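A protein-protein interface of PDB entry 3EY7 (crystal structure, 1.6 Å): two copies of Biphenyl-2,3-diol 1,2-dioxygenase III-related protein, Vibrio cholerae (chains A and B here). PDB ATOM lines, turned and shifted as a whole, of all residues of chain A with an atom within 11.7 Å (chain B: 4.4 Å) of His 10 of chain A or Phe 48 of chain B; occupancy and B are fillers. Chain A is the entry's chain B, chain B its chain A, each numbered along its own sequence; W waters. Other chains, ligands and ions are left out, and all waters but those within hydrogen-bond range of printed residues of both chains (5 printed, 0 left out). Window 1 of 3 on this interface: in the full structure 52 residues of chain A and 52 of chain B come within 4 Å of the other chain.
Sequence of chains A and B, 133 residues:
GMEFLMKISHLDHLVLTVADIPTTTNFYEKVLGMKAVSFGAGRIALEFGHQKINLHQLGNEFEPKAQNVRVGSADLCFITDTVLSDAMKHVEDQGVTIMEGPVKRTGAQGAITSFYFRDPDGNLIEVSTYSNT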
ATOM      1  N   MET A   6       2.484 -10.457  19.072  1.00  0.00           N
ATOM      2  CA  MET A   6       1.910  -9.172  19.459  1.00  0.00           C
ATOM      3  C   MET A   6       3.032  -8.224  19.838  1.00  0.00           C
ATOM      4  O   MET A   6       4.001  -8.634  20.478  1.00  0.00           O
ATOM      5  CB  MET A   6       0.960  -9.347  20.652  1.00  0.00           C
ATOM      6  CG  MET A   6       0.321  -8.045  21.133  1.00  0.00           C
ATOM      7  SD  MET A   6      -0.675  -7.216  19.683  1.00  0.00           S
ATOM      8  CE  MET A   6      -1.071  -5.491  20.517  1.00  0.00           C
ATOM      9  N   LYS A   7       2.884  -6.954  19.480  1.00  0.00           N
ATOM     10  CA  LYS A   7       3.932  -5.967  19.717  1.00  0.00           C
ATOM     11  C   LYS A   7       3.369  -4.548  19.637  1.00  0.00           C
ATOM     12  O   LYS A   7       2.527  -4.258  18.794  1.00  0.00           O
ATOM     13  CB  LYS A   7       5.033  -6.134  18.669  1.00  0.00           C
ATOM     14  CG  LYS A   7       6.244  -5.261  18.878  1.00  0.00           C
ATOM     15  CD  LYS A   7       7.290  -5.539  17.805  1.00  0.00           C
ATOM     16  CE  LYS A   7       8.460  -4.562  17.892  1.00  0.00           C
ATOM     17  NZ  LYS A   7       9.111  -4.544  19.238  1.00  0.00           N
ATOM     18  N   ILE A   8       3.842  -3.674  20.525  1.00  0.00           N
ATOM     19  CA  ILE A   8       3.448  -2.266  20.528  1.00  0.00           C
ATOM     20  C   ILE A   8       4.633  -1.402  20.092  1.00  0.00           C
ATOM     21  O   ILE A   8       5.776  -1.659  20.491  1.00  0.00           O
ATOM     22  CB  ILE A   8       2.977  -1.839  21.940  1.00  0.00           C
ATOM     23  CG1 ILE A   8       1.634  -2.516  22.269  1.00  0.00           C
ATOM     24  CG2 ILE A   8       2.864  -0.323  22.059  1.00  0.00           C
ATOM     25  CD1 ILE A   8       0.549  -2.258  21.236  1.00  0.00           C
ATOM     26  N   SER A   9       4.359  -0.394  19.266  1.00  0.00           N
ATOM     27  CA  SER A   9       5.402   0.512  18.790  1.00  0.00           C
ATOM     28  C   SER A   9       5.689   1.619  19.792  1.00  0.00           C
ATOM     29  O   SER A   9       6.831   1.848  20.174  1.00  0.00           O
ATOM     30  CB  SER A   9       5.009   1.131  17.442  1.00  0.00           C
ATOM     31  OG  SER A   9       5.870   2.216  17.092  1.00  0.00           O
ATOM     32  N   HIS A  10       4.636   2.322  20.203  1.00  0.00           N
ATOM     33  CA  HIS A  10       4.797   3.490  21.054  1.00  0.00           C
ATOM     34  C   HIS A  10       3.464   3.957  21.614  1.00  0.00           C
ATOM     35  O   HIS A  10       2.411   3.415  21.254  1.00  0.00           O
ATOM     36  CB  HIS A  10       5.458   4.637  20.293  1.00  0.00           C
ATOM     37  CG  HIS A  10       4.650   5.191  19.153  1.00  0.00           C
ATOM     38  ND1 HIS A  10       4.603   4.602  17.906  1.00  0.00           N
ATOM     39  CD2 HIS A  10       3.897   6.313  19.068  1.00  0.00           C
ATOM     40  CE1 HIS A  10       3.844   5.332  17.108  1.00  0.00           C
ATOM     41  NE2 HIS A  10       3.410   6.380  17.787  1.00  0.00           N
ATOM     42  N   LEU A  11       3.521   4.971  22.476  1.00  0.00           N
ATOM     43  CA  LEU A  11       2.320   5.583  23.037  1.00  0.00           C
ATOM     44  C   LEU A  11       1.908   6.765  22.174  1.00  0.00           C
ATOM     45  O   LEU A  11       2.706   7.668  21.906  1.00  0.00           O
ATOM     46  CB  LEU A  11       2.573   6.036  24.479  1.00  0.00           C
ATOM     47  CG  LEU A  11       1.369   6.578  25.243  1.00  0.00           C
ATOM     48  CD1 LEU A  11       1.424   6.101  26.685  1.00  0.00           C
ATOM     49  CD2 LEU A  11       1.286   8.089  25.176  1.00  0.00           C
ATOM     50  N   ASP A  12       0.656   6.769  21.725  1.00  0.00           N
ATOM     51  CA  ASP A  12       0.196   7.846  20.880  1.00  0.00           C
ATOM     52  C   ASP A  12      -0.264   9.023  21.728  1.00  0.00           C
ATOM     53  O   ASP A  12       0.071  10.172  21.465  1.00  0.00           O
ATOM     54  CB  ASP A  12      -0.961   7.389  19.994  1.00  0.00           C
ATOM     55  CG  ASP A  12      -1.375   8.455  19.014  1.00  0.00           C
ATOM     56  OD1 ASP A  12      -0.695   8.572  17.983  1.00  0.00           O
ATOM     57  OD2 ASP A  12      -2.359   9.193  19.278  1.00  0.00           O
ATOM     58  N   HIS A  13      -1.087   8.713  22.727  1.00  0.00           N
ATOM     59  CA  HIS A  13      -1.638   9.734  23.600  1.00  0.00           C
ATOM     60  C   HIS A  13      -2.144   9.122  24.883  1.00  0.00           C
ATOM     61  O   HIS A  13      -2.237   7.909  24.998  1.00  0.00           O
ATOM     62  CB  HIS A  13      -2.745  10.549  22.912  1.00  0.00           C
ATOM     63  CG  HIS A  13      -3.984   9.770  22.569  1.00  0.00           C
ATOM     64  ND1 HIS A  13      -4.197   9.229  21.318  1.00  0.00           N
ATOM     65  CD2 HIS A  13      -5.108   9.526  23.283  1.00  0.00           C
ATOM     66  CE1 HIS A  13      -5.386   8.643  21.290  1.00  0.00           C
ATOM     67  NE2 HIS A  13      -5.963   8.816  22.465  1.00  0.00           N
ATOM     68  N   LEU A  14      -2.393   9.977  25.871  1.00  0.00           N
ATOM     69  CA  LEU A  14      -3.069   9.570  27.096  1.00  0.00           C
ATOM     70  C   LEU A  14      -4.056  10.663  27.483  1.00  0.00           C
ATOM     71  O   LEU A  14      -3.975  11.795  26.987  1.00  0.00           O
ATOM     72  CB  LEU A  14      -2.061   9.307  28.221  1.00  0.00           C
ATOM     73  CG  LEU A  14      -1.171  10.466  28.675  1.00  0.00           C
ATOM     74  CD1 LEU A  14      -1.889  11.379  29.672  1.00  0.00           C
ATOM     75  CD2 LEU A  14       0.080   9.879  29.305  1.00  0.00           C
ATOM     76  N   PHE A  48       2.728  17.727  21.529  1.00  0.00           N
ATOM     77  CA  PHE A  48       4.194  17.792  21.580  1.00  0.00           C
ATOM     78  C   PHE A  48       4.786  16.659  20.749  1.00  0.00           C
ATOM     79  O   PHE A  48       4.275  15.540  20.758  1.00  0.00           O
ATOM     80  CB  PHE A  48       4.685  17.704  23.027  1.00  0.00           C
ATOM     81  CG  PHE A  48       4.190  16.501  23.758  1.00  0.00           C
ATOM     82  CD1 PHE A  48       2.929  16.502  24.346  1.00  0.00           C
ATOM     83  CD2 PHE A  48       4.981  15.370  23.877  1.00  0.00           C
ATOM     84  CE1 PHE A  48       2.457  15.391  24.999  1.00  0.00           C
ATOM     85  CE2 PHE A  48       4.513  14.252  24.549  1.00  0.00           C
ATOM     86  CZ  PHE A  48       3.248  14.264  25.115  1.00  0.00           C
ATOM     87  N   GLY A  49       5.875  16.938  20.026  1.00  0.00           N
ATOM     88  CA  GLY A  49       6.454  15.929  19.160  1.00  0.00           C
ATOM     89  C   GLY A  49       5.412  15.229  18.302  1.00  0.00           C
ATOM     90  O   GLY A  49       4.647  15.890  17.583  1.00  0.00           O
ATOM     91  N   HIS A  50       5.378  13.900  18.371  1.00  0.00           N
ATOM     92  CA  HIS A  50       4.376  13.105  17.655  1.00  0.00           C
ATOM     93  C   HIS A  50       3.364  12.440  18.580  1.00  0.00           C
ATOM     94  O   HIS A  50       2.817  11.374  18.265  1.00  0.00           O
ATOM     95  CB  HIS A  50       5.034  12.034  16.793  1.00  0.00           C
ATOM     96  CG  HIS A  50       5.768  12.590  15.612  1.00  0.00           C
ATOM     97  ND1 HIS A  50       6.880  11.982  15.072  1.00  0.00           N
ATOM     98  CD2 HIS A  50       5.563  13.715  14.886  1.00  0.00           C
ATOM     99  CE1 HIS A  50       7.318  12.700  14.051  1.00  0.00           C
ATOM    100  NE2 HIS A  50       6.537  13.756  13.918  1.00  0.00           N
ATOM    101  N   GLN A  51       3.118  13.084  19.719  1.00  0.00           N
ATOM    102  CA  GLN A  51       2.213  12.583  20.740  1.00  0.00           C
ATOM    103  C   GLN A  51       1.279  13.709  21.188  1.00  0.00           C
ATOM    104  O   GLN A  51       1.434  14.873  20.780  1.00  0.00           O
ATOM    105  CB  GLN A  51       3.015  12.066  21.946  1.00  0.00           C
ATOM    106  CG  GLN A  51       3.863  10.824  21.641  1.00  0.00           C
ATOM    107  CD  GLN A  51       4.786  10.461  22.776  1.00  0.00           C
ATOM    108  OE1 GLN A  51       5.614  11.278  23.192  1.00  0.00           O
ATOM    109  NE2 GLN A  51       4.658   9.228  23.288  1.00  0.00           N
ATOM    110  N   LYS A  52       0.296  13.369  22.019  1.00  0.00           N
ATOM    111  CA  LYS A  52      -0.510  14.409  22.640  1.00  0.00           C
ATOM    112  C   LYS A  52      -1.095  13.927  23.946  1.00  0.00           C
ATOM    113  O   LYS A  52      -1.108  12.734  24.237  1.00  0.00           O
ATOM    114  CB  LYS A  52      -1.657  14.872  21.724  1.00  0.00           C
ATOM    115  CG  LYS A  52      -2.763  13.819  21.498  1.00  0.00           C
ATOM    116  CD  LYS A  52      -3.941  14.431  20.729  1.00  0.00           C
ATOM    117  CE  LYS A  52      -4.996  13.372  20.414  1.00  0.00           C
ATOM    118  NZ  LYS A  52      -6.315  13.993  20.138  1.00  0.00           N
ATOM    119  N   ILE A  53      -1.567  14.887  24.730  1.00  0.00           N
ATOM    120  CA  ILE A  53      -2.298  14.592  25.946  1.00  0.00           C
ATOM    121  C   ILE A  53      -3.719  15.127  25.776  1.00  0.00           C
ATOM    122  O   ILE A  53      -3.907  16.325  25.577  1.00  0.00           O
ATOM    123  CB  ILE A  53      -1.620  15.260  27.160  1.00  0.00           C
ATOM    124  CG1 ILE A  53      -0.295  14.544  27.458  1.00  0.00           C
ATOM    125  CG2 ILE A  53      -2.542  15.213  28.361  1.00  0.00           C
ATOM    126  CD1 ILE A  53       0.568  15.218  28.495  1.00  0.00           C
ATOM    127  N   ASP A  75       2.075  10.731  36.568  1.00  0.00           N
ATOM    128  CA  ASP A  75       3.481  10.806  36.978  1.00  0.00           C
ATOM    129  C   ASP A  75       4.256  10.579  35.675  1.00  0.00           C
ATOM    130  O   ASP A  75       4.389   9.453  35.197  1.00  0.00           O
ATOM    131  CB  ASP A  75       3.705   9.695  38.017  1.00  0.00           C
ATOM    132  CG  ASP A  75       5.118   9.625  38.560  1.00  0.00           C
ATOM    133  OD1 ASP A  75       6.054  10.175  37.943  1.00  0.00           O
ATOM    134  OD2 ASP A  75       5.297   8.955  39.625  1.00  0.00           O
ATOM    135  N   LEU A  76       4.725  11.674  35.085  1.00  0.00           N
ATOM    136  CA  LEU A  76       5.153  11.681  33.688  1.00  0.00           C
ATOM    137  C   LEU A  76       6.579  12.155  33.553  1.00  0.00           C
ATOM    138  O   LEU A  76       6.978  13.118  34.206  1.00  0.00           O
ATOM    139  CB  LEU A  76       4.268  12.650  32.915  1.00  0.00           C
ATOM    140  CG  LEU A  76       2.761  12.420  32.998  1.00  0.00           C
ATOM    141  CD1 LEU A  76       2.042  13.478  32.183  1.00  0.00           C
ATOM    142  CD2 LEU A  76       2.362  11.005  32.518  1.00  0.00           C
ATOM    143  N   CYS A  77       7.350  11.515  32.677  1.00  0.00           N
ATOM    144  CA  CYS A  77       8.705  11.983  32.404  1.00  0.00           C
ATOM    145  C   CYS A  77       8.831  12.339  30.934  1.00  0.00           C
ATOM    146  O   CYS A  77       8.652  11.476  30.068  1.00  0.00           O
ATOM    147  CB  CYS A  77       9.716  10.890  32.756  1.00  0.00           C
ATOM    148  SG  CYS A  77      11.415  11.235  32.162  1.00  0.00           S
ATOM    149  N   GLY A 107      16.023   6.495  32.601  1.00  0.00           N
ATOM    150  CA  GLY A 107      15.022   6.592  31.552  1.00  0.00           C
ATOM    151  C   GLY A 107      14.843   5.257  30.854  1.00  0.00           C
ATOM    152  O   GLY A 107      15.549   4.290  31.167  1.00  0.00           O
ATOM    153  N   ALA A 108      13.906   5.189  29.903  1.00  0.00           N
ATOM    154  CA  ALA A 108      13.673   3.955  29.151  1.00  0.00           C
ATOM    155  C   ALA A 108      14.907   3.422  28.418  1.00  0.00           C
ATOM    156  O   ALA A 108      15.040   2.217  28.213  1.00  0.00           O
ATOM    157  CB  ALA A 108      12.504   4.137  28.144  1.00  0.00           C
ATOM    158  N   GLN A 109      15.789   4.326  27.992  1.00  0.00           N
ATOM    159  CA  GLN A 109      16.893   3.936  27.113  1.00  0.00           C
ATOM    160  C   GLN A 109      18.244   4.143  27.768  1.00  0.00           C
ATOM    161  O   GLN A 109      19.272   4.085  27.097  1.00  0.00           O
ATOM    162  CB  GLN A 109      16.822   4.682  25.772  1.00  0.00           C
ATOM    163  CG  GLN A 109      15.478   4.476  25.061  1.00  0.00           C
ATOM    164  CD  GLN A 109      15.469   5.037  23.665  1.00  0.00           C
ATOM    165  OE1 GLN A 109      16.148   4.520  22.782  1.00  0.00           O
ATOM    166  NE2 GLN A 109      14.702   6.108  23.454  1.00  0.00           N
ATOM    167  N   GLY A 110      18.236   4.370  29.072  1.00  0.00           N
ATOM    168  CA  GLY A 110      19.476   4.512  29.811  1.00  0.00           C
ATOM    169  C   GLY A 110      19.423   5.658  30.803  1.00  0.00           C
ATOM    170  O   GLY A 110      18.358   6.172  31.113  1.00  0.00           O
ATOM    171  N   TYR A 130      18.779  12.915  27.959  1.00  0.00           N
ATOM    172  CA  TYR A 130      19.751  11.835  27.869  1.00  0.00           C
ATOM    173  C   TYR A 130      21.190  12.360  27.751  1.00  0.00           C
ATOM    174  O   TYR A 130      22.148  11.592  27.846  1.00  0.00           O
ATOM    175  CB  TYR A 130      19.418  10.913  26.699  1.00  0.00           C
ATOM    176  CG  TYR A 130      18.339   9.922  27.036  1.00  0.00           C
ATOM    177  CD1 TYR A 130      18.644   8.766  27.718  1.00  0.00           C
ATOM    178  CD2 TYR A 130      17.014  10.154  26.685  1.00  0.00           C
ATOM    179  CE1 TYR A 130      17.682   7.850  28.044  1.00  0.00           C
ATOM    180  CE2 TYR A 130      16.021   9.240  27.010  1.00  0.00           C
ATOM    181  CZ  TYR A 130      16.366   8.084  27.694  1.00  0.00           C
ATOM    182  OH  TYR A 130      15.402   7.150  28.037  1.00  0.00           O
ATOM    183  N   MET B  34       4.538  -6.911  25.767  1.00  0.00           N
ATOM    184  CA  MET B  34       5.581  -6.070  26.346  1.00  0.00           C
ATOM    185  C   MET B  34       6.592  -6.911  27.116  1.00  0.00           C
ATOM    186  O   MET B  34       6.337  -8.076  27.448  1.00  0.00           O
ATOM    187  CB  MET B  34       4.968  -4.982  27.248  1.00  0.00           C
ATOM    188  CG  MET B  34       4.052  -4.035  26.491  1.00  0.00           C
ATOM    189  SD  MET B  34       3.497  -2.515  27.584  1.00  0.00           S
ATOM    190  CE  MET B  34       2.425  -1.593  26.227  1.00  0.00           C
ATOM    191  N   LEU B  46       7.683  -2.073  32.247  1.00  0.00           N
ATOM    192  CA  LEU B  46       7.268  -2.780  31.046  1.00  0.00           C
ATOM    193  C   LEU B  46       7.769  -1.997  29.847  1.00  0.00           C
ATOM    194  O   LEU B  46       7.435  -0.826  29.699  1.00  0.00           O
ATOM    195  CB  LEU B  46       5.747  -2.855  30.995  1.00  0.00           C
ATOM    196  CG  LEU B  46       5.165  -3.831  32.017  1.00  0.00           C
ATOM    197  CD1 LEU B  46       3.701  -3.486  32.304  1.00  0.00           C
ATOM    198  CD2 LEU B  46       5.317  -5.234  31.442  1.00  0.00           C
ATOM    199  N   GLU B  47       8.563  -2.638  28.988  1.00  0.00           N
ATOM    200  CA  GLU B  47       9.103  -1.968  27.808  1.00  0.00           C
ATOM    201  C   GLU B  47       8.253  -2.208  26.575  1.00  0.00           C
ATOM    202  O   GLU B  47       7.799  -3.321  26.325  1.00  0.00           O
ATOM    203  CB  GLU B  47      10.527  -2.438  27.506  1.00  0.00           C
ATOM    204  CG  GLU B  47      11.536  -2.168  28.616  1.00  0.00           C
ATOM    205  CD  GLU B  47      12.941  -2.631  28.254  1.00  0.00           C
ATOM    206  OE1 GLU B  47      13.082  -3.507  27.365  1.00  0.00           O
ATOM    207  OE2 GLU B  47      13.902  -2.121  28.862  1.00  0.00           O
ATOM    208  N   PHE B  48       8.041  -1.146  25.820  1.00  0.00           N
ATOM    209  CA  PHE B  48       7.394  -1.227  24.517  1.00  0.00           C
ATOM    210  C   PHE B  48       8.152  -0.295  23.600  1.00  0.00           C
ATOM    211  O   PHE B  48       8.407   0.847  23.949  1.00  0.00           O
ATOM    212  CB  PHE B  48       5.899  -0.854  24.617  1.00  0.00           C
ATOM    213  CG  PHE B  48       5.645   0.505  25.210  1.00  0.00           C
ATOM    214  CD1 PHE B  48       5.568   0.683  26.588  1.00  0.00           C
ATOM    215  CD2 PHE B  48       5.499   1.614  24.390  1.00  0.00           C
ATOM    216  CE1 PHE B  48       5.354   1.956  27.130  1.00  0.00           C
ATOM    217  CE2 PHE B  48       5.286   2.871  24.925  1.00  0.00           C
ATOM    218  CZ  PHE B  48       5.208   3.039  26.300  1.00  0.00           C
ATOM    219  N   GLY B  49       8.557  -0.780  22.435  1.00  0.00           N
ATOM    220  CA  GLY B  49       9.384   0.038  21.564  1.00  0.00           C
ATOM    221  C   GLY B  49      10.563   0.587  22.343  1.00  0.00           C
ATOM    222  O   GLY B  49      11.298  -0.170  22.995  1.00  0.00           O
ATOM    223  N   HIS B  50      10.724   1.905  22.308  1.00  0.00           N
ATOM    224  CA  HIS B  50      11.840   2.542  22.994  1.00  0.00           C
ATOM    225  C   HIS B  50      11.464   3.313  24.254  1.00  0.00           C
ATOM    226  O   HIS B  50      12.286   4.030  24.811  1.00  0.00           O
ATOM    227  CB  HIS B  50      12.615   3.412  22.009  1.00  0.00           C
ATOM    228  CG  HIS B  50      13.075   2.649  20.806  1.00  0.00           C
ATOM    229  ND1 HIS B  50      13.898   1.548  20.905  1.00  0.00           N
ATOM    230  CD2 HIS B  50      12.798   2.799  19.490  1.00  0.00           C
ATOM    231  CE1 HIS B  50      14.123   1.063  19.697  1.00  0.00           C
ATOM    232  NE2 HIS B  50      13.464   1.800  18.822  1.00  0.00           N
ATOM    233  N   GLN B  51      10.229   3.136  24.712  1.00  0.00           N
ATOM    234  CA  GLN B  51       9.771   3.785  25.948  1.00  0.00           C
ATOM    235  C   GLN B  51       9.332   2.724  26.950  1.00  0.00           C
ATOM    236  O   GLN B  51       9.527   1.523  26.713  1.00  0.00           O
ATOM    237  CB  GLN B  51       8.652   4.782  25.629  1.00  0.00           C
ATOM    238  CG  GLN B  51       9.164   6.062  24.969  1.00  0.00           C
ATOM    239  CD  GLN B  51       9.421   5.905  23.488  1.00  0.00           C
ATOM    240  OE1 GLN B  51       8.533   5.486  22.742  1.00  0.00           O
ATOM    241  NE2 GLN B  51      10.626   6.272  23.035  1.00  0.00           N
ATOM    242  N   LYS B  52       8.749   3.139  28.070  1.00  0.00           N
ATOM    243  CA  LYS B  52       8.359   2.152  29.064  1.00  0.00           C
ATOM    244  C   LYS B  52       7.315   2.675  30.017  1.00  0.00           C
ATOM    245  O   LYS B  52       7.049   3.875  30.074  1.00  0.00           O
ATOM    246  CB  LYS B  52       9.584   1.683  29.868  1.00  0.00           C
ATOM    247  CG  LYS B  52      10.180   2.742  30.808  1.00  0.00           C
ATOM    248  CD  LYS B  52      11.230   2.136  31.702  1.00  0.00           C
ATOM    249  CE  LYS B  52      11.907   3.190  32.570  1.00  0.00           C
ATOM    250  NZ  LYS B  52      12.538   2.547  33.772  1.00  0.00           N
ATOM    251  N   ILE B  53       6.721   1.745  30.754  1.00  0.00           N
ATOM    252  CA  ILE B  53       5.850   2.077  31.868  1.00  0.00           C
ATOM    253  C   ILE B  53       6.492   1.548  33.132  1.00  0.00           C
ATOM    254  O   ILE B  53       6.785   0.355  33.222  1.00  0.00           O
ATOM    255  CB  ILE B  53       4.493   1.423  31.695  1.00  0.00           C
ATOM    256  CG1 ILE B  53       3.787   2.042  30.483  1.00  0.00           C
ATOM    257  CG2 ILE B  53       3.636   1.583  32.978  1.00  0.00           C
ATOM    258  CD1 ILE B  53       2.453   1.406  30.162  1.00  0.00           C
ATOM    259  N   PHE B  78      -2.047   3.142  22.553  1.00  0.00           N
ATOM    260  CA  PHE B  78      -0.795   2.622  21.995  1.00  0.00           C
ATOM    261  C   PHE B  78      -0.964   2.322  20.530  1.00  0.00           C
ATOM    262  O   PHE B  78      -1.997   1.797  20.109  1.00  0.00           O
ATOM    263  CB  PHE B  78      -0.401   1.314  22.657  1.00  0.00           C
ATOM    264  CG  PHE B  78      -0.101   1.433  24.109  1.00  0.00           C
ATOM    265  CD1 PHE B  78      -1.049   1.090  25.047  1.00  0.00           C
ATOM    266  CD2 PHE B  78       1.134   1.864  24.538  1.00  0.00           C
ATOM    267  CE1 PHE B  78      -0.773   1.174  26.403  1.00  0.00           C
ATOM    268  CE2 PHE B  78       1.426   1.953  25.912  1.00  0.00           C
ATOM    269  CZ  PHE B  78       0.464   1.621  26.834  1.00  0.00           C
ATOM    270  N   ILE B  79       0.073   2.624  19.762  1.00  0.00           N
ATOM    271  CA  ILE B  79       0.115   2.293  18.350  1.00  0.00           C
ATOM    272  C   ILE B  79       0.792   0.935  18.187  1.00  0.00           C
ATOM    273  O   ILE B  79       1.826   0.663  18.800  1.00  0.00           O
ATOM    274  CB  ILE B  79       0.934   3.333  17.564  1.00  0.00           C
ATOM    275  CG1 ILE B  79       0.301   4.732  17.686  1.00  0.00           C
ATOM    276  CG2 ILE B  79       1.115   2.879  16.120  1.00  0.00           C
ATOM    277  CD1 ILE B  79      -1.154   4.809  17.295  1.00  0.00           C
HETATM  278  O   HOH W   1      12.664   7.422  25.041  1.00  0.00           O
HETATM  279  O   HOH W   2       7.878  -3.302  21.494  1.00  0.00           O
HETATM  280  O   HOH W   3      13.730   0.424  29.989  1.00  0.00           O
HETATM  281  O   HOH W   4       8.862   3.592  20.931  1.00  0.00           O
HETATM  282  O   HOH W   5       5.895   6.106  23.429  1.00  0.00           O
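Water W4 lies within hydrogen-bond range of the side-chain amide oxygen (OE1) of Gln 51 of chain B (2.6 Å), the backbone carbonyl oxygen (O) of Ser 9 of chain A (2.8 Å) and the backbone NH (N) of His 50 of chain B (2.9 Å). Water W2 lies within hydrogen-bond range of N of Gly 49 of chain B (2.8 Å), O of Ile 8 of chain A (2.9 Å) and NZ of Lys 7 of chain A (2.9 Å). Water W3 bridges the side-chain carboxylate of Glu 47 of chain B (2.8 Å) and the backbone carbonyl oxygen of Ala 108 of chain A (2.8 Å). Water W5 lies within hydrogen-bond range of the side-chain amide oxygen of Gln 51 of chain B (2.8 Å), the backbone NH of Leu 11 of chain A (2.8 Å) and the side-chain amide nitrogen of Gln 51 of chain A (3.4 Å). Water W1 lies within hydrogen-bond range of the side-chain amide nitrogen of Gln 109 of chain A (2.9 Å), the side-chain amide nitrogen of Gln 51 of chain B (3.1 Å) and the backbone carbonyl oxygen of His 50 of chain B (3.4 Å).
Positions printed for both chains: 48, 49, 50, 51, 52 and 53.
The side-chain hydroxyl (OG) of Ser 9 of chain A sits at hydrogen-bond distance from a ring nitrogen (ND1) of His 10 of chain A (2.8 Å). The backbone carbonyl oxygen (O) of Leu 11 of chain A is in hydrogen-bond range of the side-chain amide nitrogen (NE2) of Gln 51 of chain A (2.9 Å). OD2 of Asp 12 of chain A lies within hydrogen-bond range of ND1 of His 13 of chain A, 2.7 Å away. N of Lys 52 of chain A sits at hydrogen-bond distance from O of Asp 12 of chain A (3.3 Å). The backbone NH (N) of Ala 108 of chain A lies within hydrogen-bond range of the side-chain hydroxyl (OH) of Tyr 130 of chain A (3.1 Å). The backbone NH of Gln 109 of chain A sits at hydrogen-bond distance from the side-chain hydroxyl of Tyr 130 of chain A (2.9 Å).
Among the printed residues, merely in contact across the chains: Ile 8 of chain A with Gly 49 of chain B, Ile 8 of chain A with Phe 78 of chain B, Ile 8 of chain A with Ile 79 of chain B, Ser 9 of chain A with Gly 49 of chain B, His 10 of chain A with Phe 48 of chain B, His 10 of chain A with Phe 78 of chain B, Leu 11 of chain A with Phe 48 of chain B, Asp 12 of chain A with Ile 79 of chain B, Gly 107 of chain A with Lys 52 of chain B, Ala 108 of chain A with His 50 of chain B, Ala 108 of chain A with Gln 51 of chain B and Ala 108 of chain A with Lys 52 of chain B.
The side-chain amide nitrogen of Gln 109 of chain A sits close to the backbone carbonyl oxygen of His 50 of chain B. The backbone carbonyl oxygen of Ile 79 of chain B is in hydrogen-bond range of the backbone NH of Ser 9 of chain A, 2.8 Å away. The backbone NH (N) of Ile 79 of chain B lies within hydrogen-bond range of the backbone carbonyl oxygen (O) of His 10 of chain A, 2.9 Å away.
Of the 11 printed residues of chain B, 7 touch a printed residue of chain A. Printed residues of chain A that touch a printed residue of chain B: Ile 8, Ser 9, His 10, Leu 11, Asp 12, Gly 107, Ala 108 and Gln 109. Hydrophobic or aromatic side chains of chain A within 4 Å of the printed part of chain B: Ile 8, His 10 and Ala 108. Among the printed residues, no Asp or Glu carboxylate lies within 4 Å of a Lys or Arg side-chain nitrogen of the other chain.
Of chain B, only Phe 48, Phe 78 and Ile 79 come within 4 Å of His 10 of chain A. Of the printed residues of chain A, Phe 48 of chain B touches His 10 (3.9 Å) and Leu 11 (3.7 Å). No residue of chain A comes within 4 Å of Glu 47 of chain B. Gly 49 of chain B touches just these residues of chain A: Ile 8 (3.5 Å) and Ser 9 (3.4 Å). Gln 51 of chain B touches just one residue of chain A: Ala 108. No residue of chain A comes within 4 Å of Ile 53 of chain B. Ile 79 of chain B touches just these residues of chain A: Ile 8, Ser 9, His 10 and Asp 12. Of the printed residues of chain B, Asp 12 of chain A touches Ile 79. Printed residues of chain B within 4 Å of Ala 108 of chain A: His 50, Gln 51 and Lys 52. Met 6 of chain A touches none of the printed residues of chain B. Leu 14 of chain A touches none of the printed residues of chain B. The nearest residue of chain B that does not touch His 10 of chain A is Gln 51 of chain B (4.02 Å). The nearest printed residue of chain A that does not touch Phe 48 of chain B is Ile 8 of chain A (4.005 Å).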
